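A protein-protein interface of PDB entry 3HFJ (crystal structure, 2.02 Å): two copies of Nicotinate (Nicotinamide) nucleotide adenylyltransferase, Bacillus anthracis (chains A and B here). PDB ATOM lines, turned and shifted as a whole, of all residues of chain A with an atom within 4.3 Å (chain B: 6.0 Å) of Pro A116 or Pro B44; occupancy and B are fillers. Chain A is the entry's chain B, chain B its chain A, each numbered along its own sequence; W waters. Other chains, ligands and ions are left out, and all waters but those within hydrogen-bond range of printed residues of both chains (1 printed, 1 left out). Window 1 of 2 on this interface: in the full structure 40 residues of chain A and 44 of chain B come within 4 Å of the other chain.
Among the printed residues, pairs that only touch across the chains: Pro A143 with Pro B44 (3.2 Å), Lys A117 with Tyr B86 (3.3 Å), Tyr A144 with Pro B44 (3.4 Å), Pro A143 with Pro B45 (3.4 Å), Pro A143 with His B46 (3.6 Å), Pro A116 with Pro B44 (3.7 Å), Pro A116 with Pro B84 (3.7 Å), Tyr A144 with Lys B47 (3.9 Å), Pro A143 with Ile B43 (3.9 Å) and Trp A118 with Tyr B86 (3.9 Å).
Water W1 bridges the backbone carbonyl oxygen of Pro A143 (2.7 Å) and a ring nitrogen (NE2) of His B46 (3.4 Å).
Printed residues of chain A that touch a printed residue of chain B: Pro A116, Lys A117, Trp A118, Pro A143 and Tyr A144.
Hydrophobic or aromatic side chains of chain A within 4 Å of the printed part of chain B: Pro A116, Pro A143 and Tyr A144.
Among the printed residues, 12 pairs touch across the chains.
Among the printed residues, no Asp or Glu carboxylate lies within 4 Å of a Lys or Arg side-chain nitrogen of the other chain.
Tyr A114 touches none of the printed residues of chain B.
Of the printed residues of chain B, Pro A116 touches Pro B44 and Pro B84.
Of the printed residues of chain B, Trp A118 touches Tyr B86.
Printed residues of chain B within 4 Å of Tyr A144: Pro B44 and Lys B47.
Pro B44 touches just these residues of chain A: Pro A116 (3.7 Å), Pro A143 (3.2 Å) and Tyr A144 (3.4 Å).
Of the printed residues of chain A, Pro B45 touches Pro A143 (3.4 Å).
Ile B52 touches none of the printed residues of chain A.
The backbone carbonyl oxygen (O) of Pro A143 is in hydrogen-bond range of the backbone NH (N) of Lys B47 (2.9 Å).
NZ of Lys A117 lies within hydrogen-bond range of O of Ser B85 (2.7 Å).
No position is printed for both chains.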
ATOM      1  N   GLU A 113     -25.921 -14.262 -19.421  1.00  0.00           N
ATOM      2  CA  GLU A 113     -25.263 -13.409 -20.433  1.00  0.00           C
ATOM      3  C   GLU A 113     -24.142 -14.122 -21.213  1.00  0.00           C
ATOM      4  O   GLU A 113     -23.801 -13.718 -22.325  1.00  0.00           O
ATOM      5  CB  GLU A 113     -24.743 -12.115 -19.806  1.00  0.00           C
ATOM      6  CG  GLU A 113     -23.524 -12.275 -18.886  1.00  0.00           C
ATOM      7  CD  GLU A 113     -22.931 -10.931 -18.477  1.00  0.00           C
ATOM      8  OE1 GLU A 113     -22.910 -10.630 -17.264  1.00  0.00           O
ATOM      9  OE2 GLU A 113     -22.491 -10.166 -19.363  1.00  0.00           O
ATOM     10  N   TYR A 114     -23.598 -15.184 -20.628  1.00  0.00           N
ATOM     11  CA  TYR A 114     -22.503 -15.960 -21.216  1.00  0.00           C
ATOM     12  C   TYR A 114     -22.959 -17.193 -22.012  1.00  0.00           C
ATOM     13  O   TYR A 114     -22.130 -17.893 -22.597  1.00  0.00           O
ATOM     14  CB  TYR A 114     -21.501 -16.362 -20.125  1.00  0.00           C
ATOM     15  CG  TYR A 114     -20.802 -15.170 -19.510  1.00  0.00           C
ATOM     16  CD1 TYR A 114     -21.015 -14.827 -18.177  1.00  0.00           C
ATOM     17  CD2 TYR A 114     -19.943 -14.366 -20.279  1.00  0.00           C
ATOM     18  CE1 TYR A 114     -20.385 -13.716 -17.612  1.00  0.00           C
ATOM     19  CE2 TYR A 114     -19.304 -13.252 -19.724  1.00  0.00           C
ATOM     20  CZ  TYR A 114     -19.535 -12.936 -18.396  1.00  0.00           C
ATOM     21  OH  TYR A 114     -18.897 -11.855 -17.844  1.00  0.00           O
ATOM     22  N   LEU A 115     -24.272 -17.431 -22.077  1.00  0.00           N
ATOM     23  CA  LEU A 115     -24.804 -18.559 -22.863  1.00  0.00           C
ATOM     24  C   LEU A 115     -24.254 -18.659 -24.306  1.00  0.00           C
ATOM     25  O   LEU A 115     -23.985 -19.768 -24.764  1.00  0.00           O
ATOM     26  CB  LEU A 115     -26.351 -18.591 -22.842  1.00  0.00           C
ATOM     27  CG  LEU A 115     -27.022 -19.181 -21.590  1.00  0.00           C
ATOM     28  CD1 LEU A 115     -28.528 -18.969 -21.618  1.00  0.00           C
ATOM     29  CD2 LEU A 115     -26.706 -20.675 -21.411  1.00  0.00           C
ATOM     30  N   PRO A 116     -24.085 -17.521 -25.020  1.00  0.00           N
ATOM     31  CA  PRO A 116     -23.550 -17.607 -26.395  1.00  0.00           C
ATOM     32  C   PRO A 116     -22.138 -18.203 -26.541  1.00  0.00           C
ATOM     33  O   PRO A 116     -21.735 -18.553 -27.655  1.00  0.00           O
ATOM     34  CB  PRO A 116     -23.555 -16.147 -26.874  1.00  0.00           C
ATOM     35  CG  PRO A 116     -24.618 -15.478 -26.022  1.00  0.00           C
ATOM     36  CD  PRO A 116     -24.400 -16.121 -24.671  1.00  0.00           C
ATOM     37  N   LYS A 117     -21.418 -18.284 -25.427  1.00  0.00           N
ATOM     38  CA  LYS A 117     -20.084 -18.884 -25.331  1.00  0.00           C
ATOM     39  C   LYS A 117     -20.095 -20.367 -24.948  1.00  0.00           C
ATOM     40  O   LYS A 117     -19.038 -21.006 -24.904  1.00  0.00           O
ATOM     41  CB  LYS A 117     -19.255 -18.131 -24.284  1.00  0.00           C
ATOM     42  CG  LYS A 117     -18.992 -16.665 -24.639  1.00  0.00           C
ATOM     43  CD  LYS A 117     -18.032 -16.032 -23.652  1.00  0.00           C
ATOM     44  CE  LYS A 117     -17.751 -14.588 -23.983  1.00  0.00           C
ATOM     45  NZ  LYS A 117     -17.291 -14.411 -25.397  1.00  0.00           N
ATOM     46  N   TRP A 118     -21.259 -20.909 -24.619  1.00  0.00           N
ATOM     47  CA  TRP A 118     -21.320 -22.327 -24.253  1.00  0.00           C
ATOM     48  C   TRP A 118     -21.051 -23.190 -25.479  1.00  0.00           C
ATOM     49  O   TRP A 118     -21.506 -22.869 -26.580  1.00  0.00           O
ATOM     50  CB  TRP A 118     -22.683 -22.685 -23.673  1.00  0.00           C
ATOM     51  CG  TRP A 118     -22.905 -22.278 -22.237  1.00  0.00           C
ATOM     52  CD1 TRP A 118     -22.490 -21.125 -21.617  1.00  0.00           C
ATOM     53  CD2 TRP A 118     -23.646 -23.020 -21.252  1.00  0.00           C
ATOM     54  NE1 TRP A 118     -22.914 -21.117 -20.301  1.00  0.00           N
ATOM     55  CE2 TRP A 118     -23.626 -22.268 -20.055  1.00  0.00           C
ATOM     56  CE3 TRP A 118     -24.320 -24.253 -21.269  1.00  0.00           C
ATOM     57  CZ2 TRP A 118     -24.265 -22.701 -18.888  1.00  0.00           C
ATOM     58  CZ3 TRP A 118     -24.950 -24.691 -20.099  1.00  0.00           C
ATOM     59  CH2 TRP A 118     -24.917 -23.914 -18.928  1.00  0.00           C
ATOM     60  N   ILE A 121     -23.814 -24.176 -28.471  1.00  0.00           N
ATOM     61  CA  ILE A 121     -25.032 -23.632 -27.855  1.00  0.00           C
ATOM     62  C   ILE A 121     -26.319 -23.787 -28.683  1.00  0.00           C
ATOM     63  O   ILE A 121     -27.355 -24.169 -28.150  1.00  0.00           O
ATOM     64  CB  ILE A 121     -24.854 -22.147 -27.334  1.00  0.00           C
ATOM     65  CG1 ILE A 121     -26.045 -21.746 -26.462  1.00  0.00           C
ATOM     66  CG2 ILE A 121     -24.628 -21.140 -28.484  1.00  0.00           C
ATOM     67  CD1 ILE A 121     -26.266 -22.676 -25.255  1.00  0.00           C
ATOM     68  N   PRO A 143     -30.912 -13.128 -26.006  1.00  0.00           N
ATOM     69  CA  PRO A 143     -31.588 -13.393 -27.289  1.00  0.00           C
ATOM     70  C   PRO A 143     -32.290 -14.753 -27.345  1.00  0.00           C
ATOM     71  O   PRO A 143     -33.150 -14.976 -28.221  1.00  0.00           O
ATOM     72  CB  PRO A 143     -30.430 -13.370 -28.301  1.00  0.00           C
ATOM     73  CG  PRO A 143     -29.207 -13.723 -27.481  1.00  0.00           C
ATOM     74  CD  PRO A 143     -29.450 -13.018 -26.181  1.00  0.00           C
ATOM     75  N   TYR A 144     -31.928 -15.647 -26.421  1.00  0.00           N
ATOM     76  CA  TYR A 144     -32.428 -17.030 -26.380  1.00  0.00           C
ATOM     77  C   TYR A 144     -33.740 -17.199 -25.591  1.00  0.00           C
ATOM     78  O   TYR A 144     -33.969 -16.488 -24.619  1.00  0.00           O
ATOM     79  CB  TYR A 144     -31.355 -17.944 -25.770  1.00  0.00           C
ATOM     80  CG  TYR A 144     -30.007 -17.930 -26.477  1.00  0.00           C
ATOM     81  CD1 TYR A 144     -28.824 -17.860 -25.741  1.00  0.00           C
ATOM     82  CD2 TYR A 144     -29.912 -18.001 -27.875  1.00  0.00           C
ATOM     83  CE1 TYR A 144     -27.593 -17.875 -26.374  1.00  0.00           C
ATOM     84  CE2 TYR A 144     -28.678 -18.008 -28.511  1.00  0.00           C
ATOM     85  CZ  TYR A 144     -27.520 -17.944 -27.749  1.00  0.00           C
ATOM     86  OH  TYR A 144     -26.276 -17.956 -28.351  1.00  0.00           O
ATOM     87  N   GLN B  42     -19.875 -10.019 -28.093  1.00  0.00           N
ATOM     88  CA  GLN B  42     -20.966  -9.956 -29.063  1.00  0.00           C
ATOM     89  C   GLN B  42     -22.175 -10.711 -28.548  1.00  0.00           C
ATOM     90  O   GLN B  42     -22.042 -11.710 -27.820  1.00  0.00           O
ATOM     91  CB  GLN B  42     -20.551 -10.531 -30.423  1.00  0.00           C
ATOM     92  CG  GLN B  42     -20.176  -9.466 -31.442  1.00  0.00           C
ATOM     93  CD  GLN B  42     -21.359  -8.647 -31.921  1.00  0.00           C
ATOM     94  OE1 GLN B  42     -22.384  -8.524 -31.234  1.00  0.00           O
ATOM     95  NE2 GLN B  42     -21.220  -8.065 -33.107  1.00  0.00           N
ATOM     96  N   ILE B  43     -23.353 -10.221 -28.937  1.00  0.00           N
ATOM     97  CA  ILE B  43     -24.630 -10.824 -28.598  1.00  0.00           C
ATOM     98  C   ILE B  43     -25.293 -11.248 -29.926  1.00  0.00           C
ATOM     99  O   ILE B  43     -25.421 -10.430 -30.830  1.00  0.00           O
ATOM    100  CB  ILE B  43     -25.538  -9.814 -27.821  1.00  0.00           C
ATOM    101  CG1 ILE B  43     -24.854  -9.338 -26.516  1.00  0.00           C
ATOM    102  CG2 ILE B  43     -26.891 -10.434 -27.488  1.00  0.00           C
ATOM    103  CD1 ILE B  43     -25.622  -8.239 -25.720  1.00  0.00           C
ATOM    104  N   PRO B  44     -25.703 -12.527 -30.048  1.00  0.00           N
ATOM    105  CA  PRO B  44     -26.423 -12.949 -31.254  1.00  0.00           C
ATOM    106  C   PRO B  44     -27.814 -12.318 -31.342  1.00  0.00           C
ATOM    107  O   PRO B  44     -28.391 -11.936 -30.312  1.00  0.00           O
ATOM    108  CB  PRO B  44     -26.514 -14.482 -31.127  1.00  0.00           C
ATOM    109  CG  PRO B  44     -26.225 -14.793 -29.703  1.00  0.00           C
ATOM    110  CD  PRO B  44     -25.515 -13.625 -29.082  1.00  0.00           C
ATOM    111  N   PRO B  45     -28.345 -12.175 -32.571  1.00  0.00           N
ATOM    112  CA  PRO B  45     -29.665 -11.560 -32.712  1.00  0.00           C
ATOM    113  C   PRO B  45     -30.749 -12.300 -31.926  1.00  0.00           C
ATOM    114  O   PRO B  45     -30.659 -13.516 -31.739  1.00  0.00           O
ATOM    115  CB  PRO B  45     -29.925 -11.628 -34.225  1.00  0.00           C
ATOM    116  CG  PRO B  45     -28.549 -11.658 -34.824  1.00  0.00           C
ATOM    117  CD  PRO B  45     -27.761 -12.523 -33.877  1.00  0.00           C
ATOM    118  N   HIS B  46     -31.728 -11.545 -31.428  1.00  0.00           N
ATOM    119  CA  HIS B  46     -32.834 -12.110 -30.654  1.00  0.00           C
ATOM    120  C   HIS B  46     -33.607 -13.098 -31.514  1.00  0.00           C
ATOM    121  O   HIS B  46     -33.998 -12.773 -32.635  1.00  0.00           O
ATOM    122  CB  HIS B  46     -33.766 -11.010 -30.151  1.00  0.00           C
ATOM    123  CG  HIS B  46     -34.665 -11.443 -29.033  1.00  0.00           C
ATOM    124  ND1 HIS B  46     -34.461 -11.059 -27.723  1.00  0.00           N
ATOM    125  CD2 HIS B  46     -35.765 -12.232 -29.026  1.00  0.00           C
ATOM    126  CE1 HIS B  46     -35.401 -11.586 -26.959  1.00  0.00           C
ATOM    127  NE2 HIS B  46     -36.206 -12.302 -27.726  1.00  0.00           N
ATOM    128  N   LYS B  47     -33.807 -14.303 -30.977  1.00  0.00           N
ATOM    129  CA  LYS B  47     -34.471 -15.400 -31.691  1.00  0.00           C
ATOM    130  C   LYS B  47     -35.939 -15.103 -31.995  1.00  0.00           C
ATOM    131  O   LYS B  47     -36.484 -15.626 -32.961  1.00  0.00           O
ATOM    132  CB  LYS B  47     -34.381 -16.721 -30.901  1.00  0.00           C
ATOM    133  CG  LYS B  47     -32.971 -17.256 -30.643  1.00  0.00           C
ATOM    134  CD  LYS B  47     -32.410 -17.984 -31.837  1.00  0.00           C
ATOM    135  CE  LYS B  47     -30.968 -18.358 -31.602  1.00  0.00           C
ATOM    136  NZ  LYS B  47     -30.228 -18.459 -32.881  1.00  0.00           N
ATOM    137  N   ILE B  52     -32.202  -6.521 -28.449  1.00  0.00           N
ATOM    138  CA  ILE B  52     -30.915  -6.583 -27.772  1.00  0.00           C
ATOM    139  C   ILE B  52     -30.353  -5.162 -27.790  1.00  0.00           C
ATOM    140  O   ILE B  52     -30.725  -4.345 -28.641  1.00  0.00           O
ATOM    141  CB  ILE B  52     -29.939  -7.612 -28.399  1.00  0.00           C
ATOM    142  CG1 ILE B  52     -29.407  -7.135 -29.755  1.00  0.00           C
ATOM    143  CG2 ILE B  52     -30.595  -8.999 -28.484  1.00  0.00           C
ATOM    144  CD1 ILE B  52     -28.222  -7.949 -30.267  1.00  0.00           C
ATOM    145  N   PRO B  84     -20.675 -14.224 -31.624  1.00  0.00           N
ATOM    146  CA  PRO B  84     -19.974 -14.524 -30.365  1.00  0.00           C
ATOM    147  C   PRO B  84     -18.699 -15.329 -30.588  1.00  0.00           C
ATOM    148  O   PRO B  84     -18.622 -16.144 -31.526  1.00  0.00           O
ATOM    149  CB  PRO B  84     -20.983 -15.368 -29.575  1.00  0.00           C
ATOM    150  CG  PRO B  84     -22.303 -15.106 -30.195  1.00  0.00           C
ATOM    151  CD  PRO B  84     -22.042 -14.780 -31.642  1.00  0.00           C
ATOM    152  N   SER B  85     -17.715 -15.097 -29.716  1.00  0.00           N
ATOM    153  CA  SER B  85     -16.466 -15.848 -29.714  1.00  0.00           C
ATOM    154  C   SER B  85     -16.286 -16.658 -28.437  1.00  0.00           C
ATOM    155  O   SER B  85     -16.599 -16.180 -27.332  1.00  0.00           O
ATOM    156  CB  SER B  85     -15.259 -14.910 -29.836  1.00  0.00           C
ATOM    157  OG  SER B  85     -15.344 -14.084 -30.980  1.00  0.00           O
ATOM    158  N   TYR B  86     -15.758 -17.876 -28.582  1.00  0.00           N
ATOM    159  CA  TYR B  86     -15.190 -18.581 -27.437  1.00  0.00           C
ATOM    160  C   TYR B  86     -13.981 -17.807 -26.937  1.00  0.00           C
ATOM    161  O   TYR B  86     -13.176 -17.306 -27.725  1.00  0.00           O
ATOM    162  CB  TYR B  86     -14.721 -19.988 -27.820  1.00  0.00           C
ATOM    163  CG  TYR B  86     -15.818 -20.942 -28.240  1.00  0.00           C
ATOM    164  CD1 TYR B  86     -15.735 -21.620 -29.460  1.00  0.00           C
ATOM    165  CD2 TYR B  86     -16.915 -21.201 -27.410  1.00  0.00           C
ATOM    166  CE1 TYR B  86     -16.717 -22.519 -29.856  1.00  0.00           C
ATOM    167  CE2 TYR B  86     -17.917 -22.098 -27.801  1.00  0.00           C
ATOM    168  CZ  TYR B  86     -17.801 -22.754 -29.031  1.00  0.00           C
ATOM    169  OH  TYR B  86     -18.775 -23.638 -29.437  1.00  0.00           O
HETATM  170  O   HOH W   1     -35.720 -15.702 -27.658  1.00  0.00           O
